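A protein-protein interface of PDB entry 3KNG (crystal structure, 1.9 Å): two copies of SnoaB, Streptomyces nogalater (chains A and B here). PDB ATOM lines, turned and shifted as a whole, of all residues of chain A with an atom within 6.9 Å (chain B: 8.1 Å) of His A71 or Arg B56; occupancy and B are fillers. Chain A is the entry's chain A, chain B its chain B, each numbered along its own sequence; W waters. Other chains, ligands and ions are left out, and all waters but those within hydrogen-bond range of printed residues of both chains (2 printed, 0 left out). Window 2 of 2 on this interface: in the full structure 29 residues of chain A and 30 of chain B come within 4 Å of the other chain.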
ATOM      1  N   ASP A  13     -14.712  -5.177  26.513  1.00  0.00           N
ATOM      2  CA  ASP A  13     -16.073  -5.700  26.664  1.00  0.00           C
ATOM      3  C   ASP A  13     -17.071  -5.023  25.724  1.00  0.00           C
ATOM      4  O   ASP A  13     -18.101  -5.613  25.389  1.00  0.00           O
ATOM      5  CB  ASP A  13     -16.554  -5.595  28.118  1.00  0.00           C
ATOM      6  CG  ASP A  13     -16.120  -6.779  28.971  1.00  0.00           C
ATOM      7  OD1 ASP A  13     -15.589  -6.548  30.077  1.00  0.00           O
ATOM      8  OD2 ASP A  13     -16.311  -7.939  28.541  1.00  0.00           O
ATOM      9  N   GLU A  14     -16.762  -3.794  25.303  1.00  0.00           N
ATOM     10  CA  GLU A  14     -17.632  -3.025  24.408  1.00  0.00           C
ATOM     11  C   GLU A  14     -17.973  -3.786  23.133  1.00  0.00           C
ATOM     12  O   GLU A  14     -17.119  -4.462  22.554  1.00  0.00           O
ATOM     13  CB  GLU A  14     -16.990  -1.683  24.033  1.00  0.00           C
ATOM     14  CG  GLU A  14     -17.057  -0.610  25.116  1.00  0.00           C
ATOM     15  CD  GLU A  14     -16.648   0.773  24.625  1.00  0.00           C
ATOM     16  OE1 GLU A  14     -16.193   0.901  23.468  1.00  0.00           O
ATOM     17  OE2 GLU A  14     -16.787   1.739  25.405  1.00  0.00           O
ATOM     18  N   VAL A  15     -19.228  -3.678  22.711  1.00  0.00           N
ATOM     19  CA  VAL A  15     -19.642  -4.194  21.412  1.00  0.00           C
ATOM     20  C   VAL A  15     -20.154  -3.056  20.535  1.00  0.00           C
ATOM     21  O   VAL A  15     -20.713  -2.075  21.033  1.00  0.00           O
ATOM     22  CB  VAL A  15     -20.700  -5.333  21.514  1.00  0.00           C
ATOM     23  CG1 VAL A  15     -20.117  -6.558  22.211  1.00  0.00           C
ATOM     24  CG2 VAL A  15     -21.976  -4.858  22.209  1.00  0.00           C
ATOM     25  N   THR A  16     -19.946  -3.194  19.231  1.00  0.00           N
ATOM     26  CA  THR A  16     -20.380  -2.196  18.266  1.00  0.00           C
ATOM     27  C   THR A  16     -21.348  -2.816  17.263  1.00  0.00           C
ATOM     28  O   THR A  16     -21.008  -3.777  16.567  1.00  0.00           O
ATOM     29  CB  THR A  16     -19.175  -1.561  17.535  1.00  0.00           C
ATOM     30  OG1 THR A  16     -18.331  -0.901  18.488  1.00  0.00           O
ATOM     31  CG2 THR A  16     -19.636  -0.550  16.502  1.00  0.00           C
ATOM     32  N   TRP A  68     -22.117  -0.162  22.731  1.00  0.00           N
ATOM     33  CA  TRP A  68     -22.720  -0.629  23.973  1.00  0.00           C
ATOM     34  C   TRP A  68     -21.618  -1.091  24.919  1.00  0.00           C
ATOM     35  O   TRP A  68     -20.591  -1.598  24.465  1.00  0.00           O
ATOM     36  CB  TRP A  68     -23.694  -1.770  23.672  1.00  0.00           C
ATOM     37  CG  TRP A  68     -24.887  -1.296  22.907  1.00  0.00           C
ATOM     38  CD1 TRP A  68     -25.009  -1.189  21.549  1.00  0.00           C
ATOM     39  CD2 TRP A  68     -26.119  -0.831  23.459  1.00  0.00           C
ATOM     40  NE1 TRP A  68     -26.250  -0.694  21.223  1.00  0.00           N
ATOM     41  CE2 TRP A  68     -26.952  -0.465  22.377  1.00  0.00           C
ATOM     42  CE3 TRP A  68     -26.607  -0.694  24.766  1.00  0.00           C
ATOM     43  CZ2 TRP A  68     -28.249   0.030  22.562  1.00  0.00           C
ATOM     44  CZ3 TRP A  68     -27.895  -0.200  24.950  1.00  0.00           C
ATOM     45  CH2 TRP A  68     -28.699   0.156  23.852  1.00  0.00           C
ATOM     46  N   THR A  69     -21.825  -0.911  26.224  1.00  0.00           N
ATOM     47  CA  THR A  69     -20.812  -1.264  27.231  1.00  0.00           C
ATOM     48  C   THR A  69     -20.401  -2.734  27.165  1.00  0.00           C
ATOM     49  O   THR A  69     -19.231  -3.067  27.366  1.00  0.00           O
ATOM     50  CB  THR A  69     -21.274  -0.941  28.672  1.00  0.00           C
ATOM     51  OG1 THR A  69     -22.539  -1.563  28.925  1.00  0.00           O
ATOM     52  CG2 THR A  69     -21.390   0.563  28.885  1.00  0.00           C
ATOM     53  N   ASP A  70     -21.372  -3.600  26.888  1.00  0.00           N
ATOM     54  CA  ASP A  70     -21.136  -5.033  26.771  1.00  0.00           C
ATOM     55  C   ASP A  70     -22.255  -5.688  25.975  1.00  0.00           C
ATOM     56  O   ASP A  70     -23.254  -5.046  25.642  1.00  0.00           O
ATOM     57  CB  ASP A  70     -21.007  -5.679  28.157  1.00  0.00           C
ATOM     58  CG  ASP A  70     -22.172  -5.345  29.069  1.00  0.00           C
ATOM     59  OD1 ASP A  70     -22.023  -4.435  29.912  1.00  0.00           O
ATOM     60  OD2 ASP A  70     -23.238  -5.984  28.941  1.00  0.00           O
ATOM     61  N   HIS A  71     -22.073  -6.968  25.675  1.00  0.00           N
ATOM     62  CA  HIS A  71     -23.029  -7.724  24.887  1.00  0.00           C
ATOM     63  C   HIS A  71     -24.370  -7.907  25.598  1.00  0.00           C
ATOM     64  O   HIS A  71     -25.426  -7.852  24.962  1.00  0.00           O
ATOM     65  CB  HIS A  71     -22.435  -9.079  24.520  1.00  0.00           C
ATOM     66  CG  HIS A  71     -23.308  -9.887  23.621  1.00  0.00           C
ATOM     67  ND1 HIS A  71     -23.795 -11.127  23.971  1.00  0.00           N
ATOM     68  CD2 HIS A  71     -23.808  -9.618  22.393  1.00  0.00           C
ATOM     69  CE1 HIS A  71     -24.541 -11.596  22.988  1.00  0.00           C
ATOM     70  NE2 HIS A  71     -24.566 -10.698  22.019  1.00  0.00           N
ATOM     71  N   ASP A  72     -24.317  -8.120  26.911  1.00  0.00           N
ATOM     72  CA  ASP A  72     -25.521  -8.310  27.718  1.00  0.00           C
ATOM     73  C   ASP A  72     -26.432  -7.079  27.721  1.00  0.00           C
ATOM     74  O   ASP A  72     -27.651  -7.218  27.629  1.00  0.00           O
ATOM     75  CB  ASP A  72     -25.158  -8.737  29.146  1.00  0.00           C
ATOM     76  CG  ASP A  72     -24.765 -10.206  29.241  1.00  0.00           C
ATOM     77  OD1 ASP A  72     -25.179 -11.006  28.372  1.00  0.00           O
ATOM     78  OD2 ASP A  72     -24.044 -10.565  30.195  1.00  0.00           O
ATOM     79  N   ALA A  73     -25.841  -5.887  27.804  1.00  0.00           N
ATOM     80  CA  ALA A  73     -26.601  -4.635  27.748  1.00  0.00           C
ATOM     81  C   ALA A  73     -27.304  -4.448  26.402  1.00  0.00           C
ATOM     82  O   ALA A  73     -28.458  -4.016  26.355  1.00  0.00           O
ATOM     83  CB  ALA A  73     -25.697  -3.446  28.053  1.00  0.00           C
ATOM     84  N   PHE A  74     -26.596  -4.771  25.319  1.00  0.00           N
ATOM     85  CA  PHE A  74     -27.145  -4.726  23.962  1.00  0.00           C
ATOM     86  C   PHE A  74     -28.313  -5.703  23.809  1.00  0.00           C
ATOM     87  O   PHE A  74     -29.350  -5.346  23.246  1.00  0.00           O
ATOM     88  CB  PHE A  74     -26.033  -5.008  22.936  1.00  0.00           C
ATOM     89  CG  PHE A  74     -26.525  -5.265  21.530  1.00  0.00           C
ATOM     90  CD1 PHE A  74     -26.848  -4.209  20.680  1.00  0.00           C
ATOM     91  CD2 PHE A  74     -26.623  -6.566  21.045  1.00  0.00           C
ATOM     92  CE1 PHE A  74     -27.286  -4.451  19.376  1.00  0.00           C
ATOM     93  CE2 PHE A  74     -27.058  -6.817  19.746  1.00  0.00           C
ATOM     94  CZ  PHE A  74     -27.390  -5.758  18.912  1.00  0.00           C
ATOM     95  N   ARG A  75     -28.140  -6.924  24.319  1.00  0.00           N
ATOM     96  CA  ARG A  75     -29.177  -7.959  24.263  1.00  0.00           C
ATOM     97  C   ARG A  75     -30.429  -7.577  25.049  1.00  0.00           C
ATOM     98  O   ARG A  75     -31.550  -7.799  24.576  1.00  0.00           O
ATOM     99  CB  ARG A  75     -28.636  -9.301  24.767  1.00  0.00           C
ATOM    100  CG  ARG A  75     -27.723 -10.019  23.786  1.00  0.00           C
ATOM    101  N   ARG A  76     -30.228  -7.007  26.240  1.00  0.00           N
ATOM    102  CA  ARG A  76     -31.329  -6.586  27.100  1.00  0.00           C
ATOM    103  C   ARG A  76     -32.142  -5.453  26.465  1.00  0.00           C
ATOM    104  O   ARG A  76     -33.368  -5.415  26.591  1.00  0.00           O
ATOM    105  CB  ARG A  76     -30.809  -6.192  28.491  1.00  0.00           C
ATOM    106  CG  ARG A  76     -30.191  -7.354  29.277  1.00  0.00           C
ATOM    107  CD  ARG A  76     -29.876  -6.980  30.718  1.00  0.00           C
ATOM    108  NE  ARG A  76     -29.442  -8.132  31.507  1.00  0.00           N
ATOM    109  CZ  ARG A  76     -28.176  -8.400  31.811  1.00  0.00           C
ATOM    110  NH1 ARG A  76     -27.210  -7.594  31.395  1.00  0.00           N
ATOM    111  NH2 ARG A  76     -27.876  -9.470  32.534  1.00  0.00           N
ATOM    112  N   GLY A  99     -24.704  -6.296  11.789  1.00  0.00           N
ATOM    113  CA  GLY A  99     -23.844  -7.232  12.500  1.00  0.00           C
ATOM    114  C   GLY A  99     -23.360  -6.643  13.809  1.00  0.00           C
ATOM    115  O   GLY A  99     -23.392  -5.425  14.000  1.00  0.00           O
ATOM    116  N   LEU A 100     -22.912  -7.512  14.711  1.00  0.00           N
ATOM    117  CA  LEU A 100     -22.336  -7.082  15.981  1.00  0.00           C
ATOM    118  C   LEU A 100     -20.834  -7.360  15.995  1.00  0.00           C
ATOM    119  O   LEU A 100     -20.389  -8.447  15.618  1.00  0.00           O
ATOM    120  CB  LEU A 100     -23.037  -7.765  17.158  1.00  0.00           C
ATOM    121  CG  LEU A 100     -22.813  -7.184  18.557  1.00  0.00           C
ATOM    122  CD1 LEU A 100     -23.345  -5.758  18.678  1.00  0.00           C
ATOM    123  CD2 LEU A 100     -23.477  -8.075  19.578  1.00  0.00           C
ATOM    124  N   PHE A 101     -20.066  -6.365  16.437  1.00  0.00           N
ATOM    125  CA  PHE A 101     -18.612  -6.352  16.279  1.00  0.00           C
ATOM    126  C   PHE A 101     -17.868  -6.053  17.582  1.00  0.00           C
ATOM    127  O   PHE A 101     -18.440  -5.488  18.519  1.00  0.00           O
ATOM    128  CB  PHE A 101     -18.211  -5.283  15.245  1.00  0.00           C
ATOM    129  CG  PHE A 101     -18.720  -5.545  13.848  1.00  0.00           C
ATOM    130  CD1 PHE A 101     -20.039  -5.257  13.502  1.00  0.00           C
ATOM    131  CD2 PHE A 101     -17.871  -6.046  12.867  1.00  0.00           C
ATOM    132  CE1 PHE A 101     -20.509  -5.493  12.211  1.00  0.00           C
ATOM    133  CE2 PHE A 101     -18.331  -6.287  11.574  1.00  0.00           C
ATOM    134  CZ  PHE A 101     -19.653  -6.008  11.245  1.00  0.00           C
ATOM    135  N   THR A 102     -16.595  -6.448  17.625  1.00  0.00           N
ATOM    136  CA  THR A 102     -15.697  -6.014  18.691  1.00  0.00           C
ATOM    137  C   THR A 102     -14.556  -5.225  18.072  1.00  0.00           C
ATOM    138  O   THR A 102     -14.125  -5.503  16.950  1.00  0.00           O
ATOM    139  CB  THR A 102     -15.114  -7.185  19.511  1.00  0.00           C
ATOM    140  OG1 THR A 102     -14.421  -8.088  18.640  1.00  0.00           O
ATOM    141  CG2 THR A 102     -16.213  -7.932  20.258  1.00  0.00           C
ATOM    142  N   LEU B  53     -13.091  -3.068  13.230  1.00  0.00           N
ATOM    143  CA  LEU B  53     -14.036  -3.921  13.941  1.00  0.00           C
ATOM    144  C   LEU B  53     -14.039  -5.320  13.337  1.00  0.00           C
ATOM    145  O   LEU B  53     -13.928  -5.467  12.119  1.00  0.00           O
ATOM    146  CB  LEU B  53     -15.447  -3.326  13.855  1.00  0.00           C
ATOM    147  CG  LEU B  53     -15.695  -1.902  14.362  1.00  0.00           C
ATOM    148  CD1 LEU B  53     -17.012  -1.366  13.823  1.00  0.00           C
ATOM    149  CD2 LEU B  53     -15.672  -1.845  15.885  1.00  0.00           C
ATOM    150  N   ARG B  54     -14.153  -6.337  14.192  1.00  0.00           N
ATOM    151  CA  ARG B  54     -14.278  -7.726  13.751  1.00  0.00           C
ATOM    152  C   ARG B  54     -15.645  -8.252  14.177  1.00  0.00           C
ATOM    153  O   ARG B  54     -16.044  -8.081  15.333  1.00  0.00           O
ATOM    154  CB  ARG B  54     -13.161  -8.584  14.357  1.00  0.00           C
ATOM    155  CG  ARG B  54     -13.045  -9.993  13.786  1.00  0.00           C
ATOM    156  CD  ARG B  54     -11.944 -10.781  14.486  1.00  0.00           C
ATOM    157  NE  ARG B  54     -12.210 -10.950  15.913  1.00  0.00           N
ATOM    158  CZ  ARG B  54     -11.359 -11.505  16.771  1.00  0.00           C
ATOM    159  NH1 ARG B  54     -10.182 -11.948  16.350  1.00  0.00           N
ATOM    160  NH2 ARG B  54     -11.684 -11.617  18.052  1.00  0.00           N
ATOM    161  N   GLU B  55     -16.357  -8.890  13.252  1.00  0.00           N
ATOM    162  CA  GLU B  55     -17.677  -9.431  13.562  1.00  0.00           C
ATOM    163  C   GLU B  55     -17.556 -10.553  14.590  1.00  0.00           C
ATOM    164  O   GLU B  55     -16.759 -11.477  14.413  1.00  0.00           O
ATOM    165  CB  GLU B  55     -18.394  -9.912  12.294  1.00  0.00           C
ATOM    166  CG  GLU B  55     -19.904 -10.080  12.476  1.00  0.00           C
ATOM    167  CD  GLU B  55     -20.670 -10.276  11.175  1.00  0.00           C
ATOM    168  OE1 GLU B  55     -20.072 -10.171  10.083  1.00  0.00           O
ATOM    169  OE2 GLU B  55     -21.891 -10.532  11.250  1.00  0.00           O
ATOM    170  N   ARG B  56     -18.324 -10.444  15.675  1.00  0.00           N
ATOM    171  CA  ARG B  56     -18.374 -11.487  16.704  1.00  0.00           C
ATOM    172  C   ARG B  56     -18.802 -12.789  16.052  1.00  0.00           C
ATOM    173  O   ARG B  56     -19.695 -12.785  15.199  1.00  0.00           O
ATOM    174  CB  ARG B  56     -19.394 -11.143  17.794  1.00  0.00           C
ATOM    175  CG  ARG B  56     -18.980 -10.076  18.788  1.00  0.00           C
ATOM    176  CD  ARG B  56     -20.104  -9.815  19.791  1.00  0.00           C
ATOM    177  NE  ARG B  56     -19.885 -10.440  21.098  1.00  0.00           N
ATOM    178  CZ  ARG B  56     -20.446 -11.574  21.520  1.00  0.00           C
ATOM    179  NH1 ARG B  56     -21.273 -12.258  20.739  1.00  0.00           N
ATOM    180  NH2 ARG B  56     -20.168 -12.031  22.734  1.00  0.00           N
ATOM    181  N   ASP B  57     -18.174 -13.896  16.439  1.00  0.00           N
ATOM    182  CA  ASP B  57     -18.575 -15.222  15.946  1.00  0.00           C
ATOM    183  C   ASP B  57     -18.331 -15.448  14.451  1.00  0.00           C
ATOM    184  O   ASP B  57     -18.664 -16.511  13.918  1.00  0.00           O
ATOM    185  CB  ASP B  57     -20.042 -15.517  16.298  1.00  0.00           C
ATOM    186  CG  ASP B  57     -20.301 -15.509  17.794  1.00  0.00           C
ATOM    187  OD1 ASP B  57     -19.391 -15.877  18.570  1.00  0.00           O
ATOM    188  OD2 ASP B  57     -21.423 -15.140  18.197  1.00  0.00           O
ATOM    189  N   LYS B  58     -17.769 -14.450  13.781  1.00  0.00           N
ATOM    190  CA  LYS B  58     -17.185 -14.670  12.474  1.00  0.00           C
ATOM    191  C   LYS B  58     -15.697 -14.462  12.605  1.00  0.00           C
ATOM    192  O   LYS B  58     -15.219 -13.786  13.520  1.00  0.00           O
ATOM    193  CB  LYS B  58     -17.795 -13.763  11.405  1.00  0.00           C
ATOM    194  CG  LYS B  58     -19.250 -14.091  11.114  1.00  0.00           C
ATOM    195  CD  LYS B  58     -19.661 -13.741   9.699  1.00  0.00           C
ATOM    196  CE  LYS B  58     -21.126 -14.089   9.477  1.00  0.00           C
ATOM    197  NZ  LYS B  58     -21.582 -13.757   8.106  1.00  0.00           N
ATOM    198  N   ASP B  59     -14.969 -15.060  11.679  1.00  0.00           N
ATOM    199  CA  ASP B  59     -13.535 -15.074  11.738  1.00  0.00           C
ATOM    200  C   ASP B  59     -12.968 -14.091  10.732  1.00  0.00           C
ATOM    201  O   ASP B  59     -11.930 -13.471  10.968  1.00  0.00           O
ATOM    202  CB  ASP B  59     -13.064 -16.484  11.409  1.00  0.00           C
ATOM    203  CG  ASP B  59     -11.583 -16.668  11.604  1.00  0.00           C
ATOM    204  OD1 ASP B  59     -11.036 -16.140  12.592  1.00  0.00           O
ATOM    205  OD2 ASP B  59     -10.960 -17.354  10.770  1.00  0.00           O
ATOM    206  N   SER B  61     -14.775 -11.552   8.895  1.00  0.00           N
ATOM    207  CA  SER B  61     -15.606 -10.397   8.596  1.00  0.00           C
ATOM    208  C   SER B  61     -15.146  -9.192   9.409  1.00  0.00           C
ATOM    209  O   SER B  61     -15.186  -9.212  10.641  1.00  0.00           O
ATOM    210  CB  SER B  61     -17.074 -10.715   8.883  1.00  0.00           C
ATOM    211  OG  SER B  61     -17.883  -9.561   8.747  1.00  0.00           O
HETATM  212  O   HOH W   1     -14.965 -10.358  17.188  1.00  0.00           O
HETATM  213  O   HOH W   2     -23.210 -10.334  13.859  1.00  0.00           O
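The backbone NH (N) of Arg B56 sits at hydrogen-bond distance from the backbone carbonyl oxygen (O) of Leu A100 (2.9 Å). The backbone NH (N) of Thr A102 is in hydrogen-bond range of the backbone carbonyl oxygen (O) of Arg B54, 2.9 Å away.
No position is printed for both chains. Of the 10 pairs that touch across the chains among the printed residues, none has its exchanged pair printed and touching as well.
Thr A16 touches Leu B53. His A71 touches Arg B56 (NE2 to NH1, 3.9 Å). CA of Glu B55 touches O of Leu A100 (3.5 Å). CB of Phe A101 touches CB of Leu B53 (3.7 Å). Phe A101 touches Arg B54 (CA to O, 3.2 Å). CD2 of Phe A101 touches N of Glu B55, at 3.2 Å. CA of Leu B53 touches O of Thr A102, at 3.4 Å. Thr A102 touches Arg B56 (CG2 to CG, 3.8 Å).
Gly A99 touches none of the printed residues of chain B. Of the printed residues of chain B, Leu A100 touches Glu B55 (3.5 Å) and Arg B56 (2.9 Å). Of the printed residues of chain B, Thr A102 touches Leu B53 (3.4 Å), Arg B54 (2.9 Å) and Arg B56 (3.8 Å). Printed residues of chain A within 4 Å of Leu B53: Thr A16 (3.8 Å), Phe A101 (3.7 Å) and Thr A102 (3.4 Å). Of the printed residues of chain A, Glu B55 touches Leu A100 (3.5 Å) and Phe A101 (3.2 Å). Of the printed residues of chain A, Arg B56 touches His A71 (3.9 Å), Leu A100 (2.9 Å) and Thr A102 (3.8 Å). The nearest printed residue of chain A that does not touch Arg B56 is Val A15 (4.05 Å).
Water W1 lies within hydrogen-bond range of the side-chain hydroxyl of Thr A102 (2.7 Å), the guanidinium group of Arg B54 (3.1 Å) and the backbone carbonyl oxygen of Glu B55 (3.5 Å). Water W2 bridges OE2 of Glu B55 (2.9 Å) and N of Leu A100 (3.0 Å).
Of the 8 printed residues of chain B, 4 touch a printed residue of chain A. Hydrophobic or aromatic side chains of chain A that line the printed part of chain B: His A71, Leu A100 and Phe A101. Among the printed residues, no Asp or Glu carboxylate lies within 4 Å of a Lys or Arg side-chain nitrogen of the other chain.
O of Thr A16 lies within hydrogen-bond range of N of Phe A101, at 2.8 Å. OE1 of Glu B55 is in hydrogen-bond range of OG of Ser B61, at 2.6 Å. NH1 of Arg B56 is in salt-bridge range of OD2 of Asp B57 (3.8 Å).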
